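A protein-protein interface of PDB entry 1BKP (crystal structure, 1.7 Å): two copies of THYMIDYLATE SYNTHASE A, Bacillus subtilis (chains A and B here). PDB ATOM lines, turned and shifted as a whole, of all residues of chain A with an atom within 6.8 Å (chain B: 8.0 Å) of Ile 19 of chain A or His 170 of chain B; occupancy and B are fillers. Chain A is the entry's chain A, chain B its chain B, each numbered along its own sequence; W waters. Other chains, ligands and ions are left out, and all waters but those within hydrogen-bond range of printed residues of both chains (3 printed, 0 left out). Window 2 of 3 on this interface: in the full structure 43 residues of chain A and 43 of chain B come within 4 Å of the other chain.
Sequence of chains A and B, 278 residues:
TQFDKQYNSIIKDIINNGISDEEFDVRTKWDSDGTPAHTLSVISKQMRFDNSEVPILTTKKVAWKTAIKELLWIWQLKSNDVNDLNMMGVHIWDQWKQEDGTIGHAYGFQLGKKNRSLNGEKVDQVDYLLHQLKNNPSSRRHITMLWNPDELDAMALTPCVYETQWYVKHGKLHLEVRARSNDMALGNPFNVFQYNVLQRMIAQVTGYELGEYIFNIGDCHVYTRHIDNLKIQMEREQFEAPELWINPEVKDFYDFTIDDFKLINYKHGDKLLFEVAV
The backbone NH (N) of His 170 of chain B lies within hydrogen-bond range of the side-chain carboxylate (OE2) of Glu 23 of chain A (2.8 Å). The side-chain hydroxyl (OG) of Ser 41 of chain A is in hydrogen-bond range of the side-chain amino group (NZ) of Lys 169 of chain B.
N of Ile 19 of chain A sits at hydrogen-bond distance from O of Ser 41 of chain A (2.8 Å). N of His 174 of chain B sits at hydrogen-bond distance from O of Tyr 167 of chain B (2.8 Å).
Among the printed residues, pairs that only touch across the chains: Ile 19 of chain A with His 170 of chain B (3.4 Å), Ile 43 of chain A with His 174 of chain B (3.4 Å), Phe 24 of chain A with Val 168 of chain B (3.6 Å), Phe 24 of chain A with Pro 137 of chain B (3.6 Å), Ile 43 of chain A with Tyr 167 of chain B (3.7 Å), Ile 43 of chain A with Lys 169 of chain B (3.7 Å) and Glu 23 of chain A with Lys 169 of chain B (3.8 Å).
No residue of chain B comes within 4 Å of Gly 18 of chain A. Ser 20 of chain A touches none of the printed residues of chain B. Glu 22 of chain A touches none of the printed residues of chain B. Of the printed residues of chain B, Ile 43 of chain A touches Tyr 167 (3.7 Å), Lys 169 (3.7 Å) and His 174 (3.4 Å). Of the printed residues of chain A, Tyr 167 of chain B touches Ile 43 (3.7 Å). Of chain A, only Ile 19 and Glu 23 come within 4 Å of His 170 of chain B. The nearest residue of chain A that does not touch His 170 of chain B is Ser 20 of chain A (4.2 Å).
Of the 11 printed residues of chain B, 6 touch a printed residue of chain A. Hydrophobic or aromatic side chains of chain B that line the printed part of chain A: Pro 137, Tyr 167, His 170 and His 174. Of the 14 printed residues of chain A, 5 touch a printed residue of chain B. Hydrophobic or aromatic side chains of chain A within 4 Å of the printed part of chain B: Ile 19, Phe 24 and Ile 43.
No position is printed for both chains. Of the 9 pairs that touch across the chains among the printed residues, none has its exchanged pair printed and touching as well.
Water W2 lies within hydrogen-bond range of the side-chain carboxylate (OE1) of Glu 23 of chain A (2.6 Å), the backbone NH (N) of Gly 171 of chain B (3.0 Å) and the backbone NH (N) of His 170 of chain B (3.3 Å). Water W3 lies within hydrogen-bond range of the backbone NH of Ser 20 of chain A and a ring nitrogen (NE2) of His 170 of chain B. Water W1 lies within hydrogen-bond range of NZ of Lys 169 of chain B (3.0 Å) and OG of Ser 41 of chain A (3.5 Å).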
ATOM      1  N   ILE A  14      -1.646  25.409  29.028  1.00  0.00           N
ATOM      2  CA  ILE A  14      -2.589  24.763  28.152  1.00  0.00           C
ATOM      3  C   ILE A  14      -3.088  23.421  28.729  1.00  0.00           C
ATOM      4  O   ILE A  14      -4.341  23.132  28.764  1.00  0.00           O
ATOM      5  CB  ILE A  14      -1.939  24.540  26.712  1.00  0.00           C
ATOM      6  CG1 ILE A  14      -1.729  25.892  26.022  1.00  0.00           C
ATOM      7  CG2 ILE A  14      -2.835  23.635  25.792  1.00  0.00           C
ATOM      8  CD1 ILE A  14      -0.914  25.743  24.651  1.00  0.00           C
ATOM      9  N   ASN A  17      -5.261  24.593  31.925  1.00  0.00           N
ATOM     10  CA  ASN A  17      -6.401  25.483  31.794  1.00  0.00           C
ATOM     11  C   ASN A  17      -6.941  25.456  30.411  1.00  0.00           C
ATOM     12  O   ASN A  17      -7.888  26.205  30.091  1.00  0.00           O
ATOM     13  CB  ASN A  17      -5.896  26.903  32.028  1.00  0.00           C
ATOM     14  CG  ASN A  17      -5.370  27.094  33.411  1.00  0.00           C
ATOM     15  OD1 ASN A  17      -6.025  26.738  34.376  1.00  0.00           O
ATOM     16  ND2 ASN A  17      -4.184  27.638  33.520  1.00  0.00           N
ATOM     17  N   GLY A  18      -6.355  24.625  29.553  1.00  0.00           N
ATOM     18  CA  GLY A  18      -6.845  24.617  28.172  1.00  0.00           C
ATOM     19  C   GLY A  18      -8.279  24.136  27.966  1.00  0.00           C
ATOM     20  O   GLY A  18      -8.773  23.304  28.723  1.00  0.00           O
ATOM     21  N   ILE A  19      -8.939  24.631  26.935  1.00  0.00           N
ATOM     22  CA  ILE A  19     -10.301  24.249  26.635  1.00  0.00           C
ATOM     23  C   ILE A  19     -10.370  23.215  25.495  1.00  0.00           C
ATOM     24  O   ILE A  19      -9.729  23.364  24.449  1.00  0.00           O
ATOM     25  CB  ILE A  19     -11.112  25.534  26.255  1.00  0.00           C
ATOM     26  CG1 ILE A  19     -10.997  26.546  27.392  1.00  0.00           C
ATOM     27  CG2 ILE A  19     -12.593  25.184  25.962  1.00  0.00           C
ATOM     28  CD1 ILE A  19     -10.619  27.882  26.900  1.00  0.00           C
ATOM     29  N   SER A  20     -11.191  22.171  25.687  1.00  0.00           N
ATOM     30  CA  SER A  20     -11.267  21.127  24.718  1.00  0.00           C
ATOM     31  C   SER A  20     -12.156  21.420  23.555  1.00  0.00           C
ATOM     32  O   SER A  20     -13.107  22.096  23.727  1.00  0.00           O
ATOM     33  CB  SER A  20     -11.743  19.857  25.448  1.00  0.00           C
ATOM     34  OG  SER A  20     -12.091  18.889  24.479  1.00  0.00           O
ATOM     35  N   ASP A  21     -11.815  20.984  22.343  1.00  0.00           N
ATOM     36  CA  ASP A  21     -12.716  21.127  21.219  1.00  0.00           C
ATOM     37  C   ASP A  21     -13.641  19.950  21.026  1.00  0.00           C
ATOM     38  O   ASP A  21     -14.188  19.757  19.928  1.00  0.00           O
ATOM     39  CB  ASP A  21     -11.999  21.456  19.930  1.00  0.00           C
ATOM     40  CG  ASP A  21     -10.924  20.450  19.573  1.00  0.00           C
ATOM     41  OD1 ASP A  21     -10.850  19.426  20.264  1.00  0.00           O
ATOM     42  OD2 ASP A  21     -10.176  20.723  18.589  1.00  0.00           O
ATOM     43  N   GLU A  22     -13.808  19.149  22.084  1.00  0.00           N
ATOM     44  CA  GLU A  22     -14.722  17.948  22.029  1.00  0.00           C
ATOM     45  C   GLU A  22     -16.190  18.360  21.612  1.00  0.00           C
ATOM     46  O   GLU A  22     -16.911  17.588  21.004  1.00  0.00           O
ATOM     47  CB  GLU A  22     -14.761  17.339  23.423  1.00  0.00           C
ATOM     48  CG  GLU A  22     -13.769  16.292  23.706  1.00  0.00           C
ATOM     49  CD  GLU A  22     -13.332  16.303  25.192  1.00  0.00           C
ATOM     50  OE1 GLU A  22     -13.910  17.064  26.016  1.00  0.00           O
ATOM     51  OE2 GLU A  22     -12.363  15.579  25.522  1.00  0.00           O
ATOM     52  N   GLU A  23     -16.580  19.623  21.865  1.00  0.00           N
ATOM     53  CA  GLU A  23     -17.902  20.098  21.528  1.00  0.00           C
ATOM     54  C   GLU A  23     -18.190  20.216  20.047  1.00  0.00           C
ATOM     55  O   GLU A  23     -19.393  20.305  19.635  1.00  0.00           O
ATOM     56  CB  GLU A  23     -18.180  21.430  22.180  1.00  0.00           C
ATOM     57  CG  GLU A  23     -17.252  22.560  21.659  1.00  0.00           C
ATOM     58  CD  GLU A  23     -17.598  23.924  22.233  1.00  0.00           C
ATOM     59  OE1 GLU A  23     -18.794  24.223  22.243  1.00  0.00           O
ATOM     60  OE2 GLU A  23     -16.672  24.689  22.664  1.00  0.00           O
ATOM     61  N   PHE A  24     -17.124  20.291  19.249  1.00  0.00           N
ATOM     62  CA  PHE A  24     -17.261  20.420  17.820  1.00  0.00           C
ATOM     63  C   PHE A  24     -17.073  19.099  17.101  1.00  0.00           C
ATOM     64  O   PHE A  24     -16.464  18.162  17.656  1.00  0.00           O
ATOM     65  CB  PHE A  24     -16.224  21.458  17.304  1.00  0.00           C
ATOM     66  CG  PHE A  24     -16.347  22.820  17.988  1.00  0.00           C
ATOM     67  CD1 PHE A  24     -17.467  23.582  17.844  1.00  0.00           C
ATOM     68  CD2 PHE A  24     -15.327  23.317  18.775  1.00  0.00           C
ATOM     69  CE1 PHE A  24     -17.592  24.828  18.446  1.00  0.00           C
ATOM     70  CE2 PHE A  24     -15.432  24.596  19.410  1.00  0.00           C
ATOM     71  CZ  PHE A  24     -16.592  25.348  19.220  1.00  0.00           C
ATOM     72  N   THR A  39      -8.152  18.766  20.511  1.00  0.00           N
ATOM     73  CA  THR A  39      -7.090  19.591  21.072  1.00  0.00           C
ATOM     74  C   THR A  39      -7.564  20.343  22.287  1.00  0.00           C
ATOM     75  O   THR A  39      -8.770  20.303  22.586  1.00  0.00           O
ATOM     76  CB  THR A  39      -6.668  20.703  20.089  1.00  0.00           C
ATOM     77  OG1 THR A  39      -7.784  21.577  19.839  1.00  0.00           O
ATOM     78  CG2 THR A  39      -6.178  20.116  18.767  1.00  0.00           C
ATOM     79  N   LEU A  40      -6.614  20.756  23.122  1.00  0.00           N
ATOM     80  CA  LEU A  40      -6.827  21.697  24.242  1.00  0.00           C
ATOM     81  C   LEU A  40      -6.225  23.058  23.712  1.00  0.00           C
ATOM     82  O   LEU A  40      -5.175  23.043  23.059  1.00  0.00           O
ATOM     83  CB  LEU A  40      -6.035  21.342  25.538  1.00  0.00           C
ATOM     84  CG  LEU A  40      -6.407  20.003  26.213  1.00  0.00           C
ATOM     85  CD1 LEU A  40      -5.530  19.762  27.391  1.00  0.00           C
ATOM     86  CD2 LEU A  40      -7.865  19.996  26.597  1.00  0.00           C
ATOM     87  N   SER A  41      -6.870  24.197  23.998  1.00  0.00           N
ATOM     88  CA  SER A  41      -6.310  25.440  23.515  1.00  0.00           C
ATOM     89  C   SER A  41      -6.574  26.555  24.467  1.00  0.00           C
ATOM     90  O   SER A  41      -7.476  26.473  25.333  1.00  0.00           O
ATOM     91  CB  SER A  41      -6.917  25.778  22.148  1.00  0.00           C
ATOM     92  OG  SER A  41      -8.323  25.853  22.301  1.00  0.00           O
ATOM     93  N   VAL A  42      -5.757  27.594  24.317  1.00  0.00           N
ATOM     94  CA  VAL A  42      -5.868  28.865  25.055  1.00  0.00           C
ATOM     95  C   VAL A  42      -5.706  29.978  23.988  1.00  0.00           C
ATOM     96  O   VAL A  42      -5.285  29.736  22.846  1.00  0.00           O
ATOM     97  CB  VAL A  42      -4.836  29.089  26.149  1.00  0.00           C
ATOM     98  CG1 VAL A  42      -5.045  28.071  27.284  1.00  0.00           C
ATOM     99  CG2 VAL A  42      -3.362  29.076  25.551  1.00  0.00           C
ATOM    100  N   ILE A  43      -6.207  31.149  24.307  1.00  0.00           N
ATOM    101  CA  ILE A  43      -6.216  32.263  23.379  1.00  0.00           C
ATOM    102  C   ILE A  43      -5.244  33.354  23.757  1.00  0.00           C
ATOM    103  O   ILE A  43      -5.203  33.774  24.928  1.00  0.00           O
ATOM    104  CB  ILE A  43      -7.665  32.895  23.397  1.00  0.00           C
ATOM    105  CG1 ILE A  43      -8.697  31.941  22.748  1.00  0.00           C
ATOM    106  CG2 ILE A  43      -7.766  34.109  22.610  1.00  0.00           C
ATOM    107  CD1 ILE A  43     -10.181  32.513  23.032  1.00  0.00           C
ATOM    108  N   PRO B 137     -18.167  27.543  13.771  1.00  0.00           N
ATOM    109  CA  PRO B 137     -17.585  28.204  14.956  1.00  0.00           C
ATOM    110  C   PRO B 137     -16.183  27.883  15.369  1.00  0.00           C
ATOM    111  O   PRO B 137     -15.538  28.761  15.898  1.00  0.00           O
ATOM    112  CB  PRO B 137     -18.572  27.848  16.116  1.00  0.00           C
ATOM    113  CG  PRO B 137     -19.193  26.541  15.650  1.00  0.00           C
ATOM    114  CD  PRO B 137     -19.335  26.706  14.130  1.00  0.00           C
ATOM    115  N   TYR B 167     -12.903  34.064  18.152  1.00  0.00           N
ATOM    116  CA  TYR B 167     -12.820  32.683  18.554  1.00  0.00           C
ATOM    117  C   TYR B 167     -14.144  32.351  19.258  1.00  0.00           C
ATOM    118  O   TYR B 167     -14.715  33.140  20.032  1.00  0.00           O
ATOM    119  CB  TYR B 167     -11.734  32.467  19.625  1.00  0.00           C
ATOM    120  CG  TYR B 167     -10.416  33.137  19.314  1.00  0.00           C
ATOM    121  CD1 TYR B 167     -10.215  34.469  19.596  1.00  0.00           C
ATOM    122  CD2 TYR B 167      -9.408  32.433  18.721  1.00  0.00           C
ATOM    123  CE1 TYR B 167      -9.008  35.114  19.327  1.00  0.00           C
ATOM    124  CE2 TYR B 167      -8.157  33.067  18.384  1.00  0.00           C
ATOM    125  CZ  TYR B 167      -7.960  34.403  18.713  1.00  0.00           C
ATOM    126  OH  TYR B 167      -6.689  35.019  18.467  1.00  0.00           O
ATOM    127  N   VAL B 168     -14.598  31.124  19.035  1.00  0.00           N
ATOM    128  CA  VAL B 168     -15.844  30.713  19.669  1.00  0.00           C
ATOM    129  C   VAL B 168     -15.467  29.458  20.471  1.00  0.00           C
ATOM    130  O   VAL B 168     -14.980  28.490  19.896  1.00  0.00           O
ATOM    131  CB  VAL B 168     -16.895  30.261  18.697  1.00  0.00           C
ATOM    132  CG1 VAL B 168     -18.138  29.775  19.562  1.00  0.00           C
ATOM    133  CG2 VAL B 168     -17.298  31.355  17.682  1.00  0.00           C
ATOM    134  N   LYS B 169     -15.584  29.539  21.782  1.00  0.00           N
ATOM    135  CA  LYS B 169     -15.306  28.402  22.664  1.00  0.00           C
ATOM    136  C   LYS B 169     -16.375  28.294  23.781  1.00  0.00           C
ATOM    137  O   LYS B 169     -16.563  29.270  24.531  1.00  0.00           O
ATOM    138  CB  LYS B 169     -13.924  28.549  23.269  1.00  0.00           C
ATOM    139  CG  LYS B 169     -12.789  28.452  22.206  1.00  0.00           C
ATOM    140  CD  LYS B 169     -11.403  28.494  22.902  1.00  0.00           C
ATOM    141  CE  LYS B 169     -10.259  28.733  21.906  1.00  0.00           C
ATOM    142  NZ  LYS B 169     -10.149  27.755  20.794  1.00  0.00           N
ATOM    143  N   HIS B 170     -17.083  27.143  23.848  1.00  0.00           N
ATOM    144  CA  HIS B 170     -18.093  26.936  24.887  1.00  0.00           C
ATOM    145  C   HIS B 170     -19.155  28.008  24.872  1.00  0.00           C
ATOM    146  O   HIS B 170     -19.488  28.535  25.913  1.00  0.00           O
ATOM    147  CB  HIS B 170     -17.510  26.925  26.275  1.00  0.00           C
ATOM    148  CG  HIS B 170     -16.734  25.692  26.589  1.00  0.00           C
ATOM    149  ND1 HIS B 170     -16.009  25.554  27.757  1.00  0.00           N
ATOM    150  CD2 HIS B 170     -16.522  24.566  25.866  1.00  0.00           C
ATOM    151  CE1 HIS B 170     -15.369  24.400  27.728  1.00  0.00           C
ATOM    152  NE2 HIS B 170     -15.666  23.781  26.591  1.00  0.00           N
ATOM    153  N   GLY B 171     -19.701  28.279  23.698  1.00  0.00           N
ATOM    154  CA  GLY B 171     -20.783  29.237  23.618  1.00  0.00           C
ATOM    155  C   GLY B 171     -20.348  30.676  23.847  1.00  0.00           C
ATOM    156  O   GLY B 171     -21.230  31.541  23.883  1.00  0.00           O
ATOM    157  N   LYS B 172     -19.041  30.949  24.042  1.00  0.00           N
ATOM    158  CA  LYS B 172     -18.627  32.382  24.245  1.00  0.00           C
ATOM    159  C   LYS B 172     -17.832  32.913  23.006  1.00  0.00           C
ATOM    160  O   LYS B 172     -17.031  32.175  22.401  1.00  0.00           O
ATOM    161  CB  LYS B 172     -17.744  32.489  25.476  1.00  0.00           C
ATOM    162  CG  LYS B 172     -18.427  32.670  26.793  1.00  0.00           C
ATOM    163  CD  LYS B 172     -18.962  31.466  27.451  1.00  0.00           C
ATOM    164  CE  LYS B 172     -19.547  31.886  28.829  1.00  0.00           C
ATOM    165  NZ  LYS B 172     -20.627  30.989  29.381  1.00  0.00           N
ATOM    166  N   LEU B 173     -18.070  34.167  22.625  1.00  0.00           N
ATOM    167  CA  LEU B 173     -17.374  34.783  21.511  1.00  0.00           C
ATOM    168  C   LEU B 173     -16.297  35.685  22.065  1.00  0.00           C
ATOM    169  O   LEU B 173     -16.598  36.660  22.741  1.00  0.00           O
ATOM    170  CB  LEU B 173     -18.360  35.645  20.721  1.00  0.00           C
ATOM    171  CG  LEU B 173     -17.911  36.329  19.435  1.00  0.00           C
ATOM    172  CD1 LEU B 173     -17.471  35.241  18.475  1.00  0.00           C
ATOM    173  CD2 LEU B 173     -19.158  37.058  18.823  1.00  0.00           C
ATOM    174  N   HIS B 174     -15.045  35.360  21.752  1.00  0.00           N
ATOM    175  CA  HIS B 174     -13.852  36.127  22.223  1.00  0.00           C
ATOM    176  C   HIS B 174     -13.371  36.995  21.073  1.00  0.00           C
ATOM    177  O   HIS B 174     -13.502  36.626  19.902  1.00  0.00           O
ATOM    178  CB  HIS B 174     -12.711  35.093  22.638  1.00  0.00           C
ATOM    179  CG  HIS B 174     -13.107  34.137  23.734  1.00  0.00           C
ATOM    180  ND1 HIS B 174     -13.791  32.944  23.500  1.00  0.00           N
ATOM    181  CD2 HIS B 174     -12.926  34.193  25.081  1.00  0.00           C
ATOM    182  CE1 HIS B 174     -14.034  32.325  24.639  1.00  0.00           C
ATOM    183  NE2 HIS B 174     -13.529  33.057  25.611  1.00  0.00           N
ATOM    184  N   TYR B 208     -24.254  34.354  20.761  1.00  0.00           N
ATOM    185  CA  TYR B 208     -23.232  33.891  21.751  1.00  0.00           C
ATOM    186  C   TYR B 208     -23.115  34.754  22.942  1.00  0.00           C
ATOM    187  O   TYR B 208     -23.499  35.899  22.913  1.00  0.00           O
ATOM    188  CB  TYR B 208     -21.818  33.836  21.096  1.00  0.00           C
ATOM    189  CG  TYR B 208     -21.653  32.756  20.036  1.00  0.00           C
ATOM    190  CD1 TYR B 208     -21.692  31.390  20.366  1.00  0.00           C
ATOM    191  CD2 TYR B 208     -21.500  33.107  18.684  1.00  0.00           C
ATOM    192  CE1 TYR B 208     -21.615  30.388  19.326  1.00  0.00           C
ATOM    193  CE2 TYR B 208     -21.401  32.174  17.658  1.00  0.00           C
ATOM    194  CZ  TYR B 208     -21.462  30.818  17.976  1.00  0.00           C
ATOM    195  OH  TYR B 208     -21.421  29.961  16.899  1.00  0.00           O
ATOM    196  N   GLU B 209     -22.573  34.215  24.001  1.00  0.00           N
ATOM    197  CA  GLU B 209     -22.325  34.986  25.197  1.00  0.00           C
ATOM    198  C   GLU B 209     -20.983  35.716  24.976  1.00  0.00           C
ATOM    199  O   GLU B 209     -20.203  35.315  24.129  1.00  0.00           O
ATOM    200  CB  GLU B 209     -22.148  34.042  26.380  1.00  0.00           C
ATOM    201  CG  GLU B 209     -23.571  33.676  26.935  1.00  0.00           C
ATOM    202  CD  GLU B 209     -23.540  33.059  28.304  1.00  0.00           C
ATOM    203  OE1 GLU B 209     -22.509  33.187  29.017  1.00  0.00           O
ATOM    204  OE2 GLU B 209     -24.568  32.448  28.670  1.00  0.00           O
HETATM  205  O   HOH W   1     -11.484  25.102  21.094  1.00  0.00           O
HETATM  206  O   HOH W   2     -19.120  26.610  21.324  1.00  0.00           O
HETATM  207  O   HOH W   3     -13.012  22.162  27.950  1.00  0.00           O
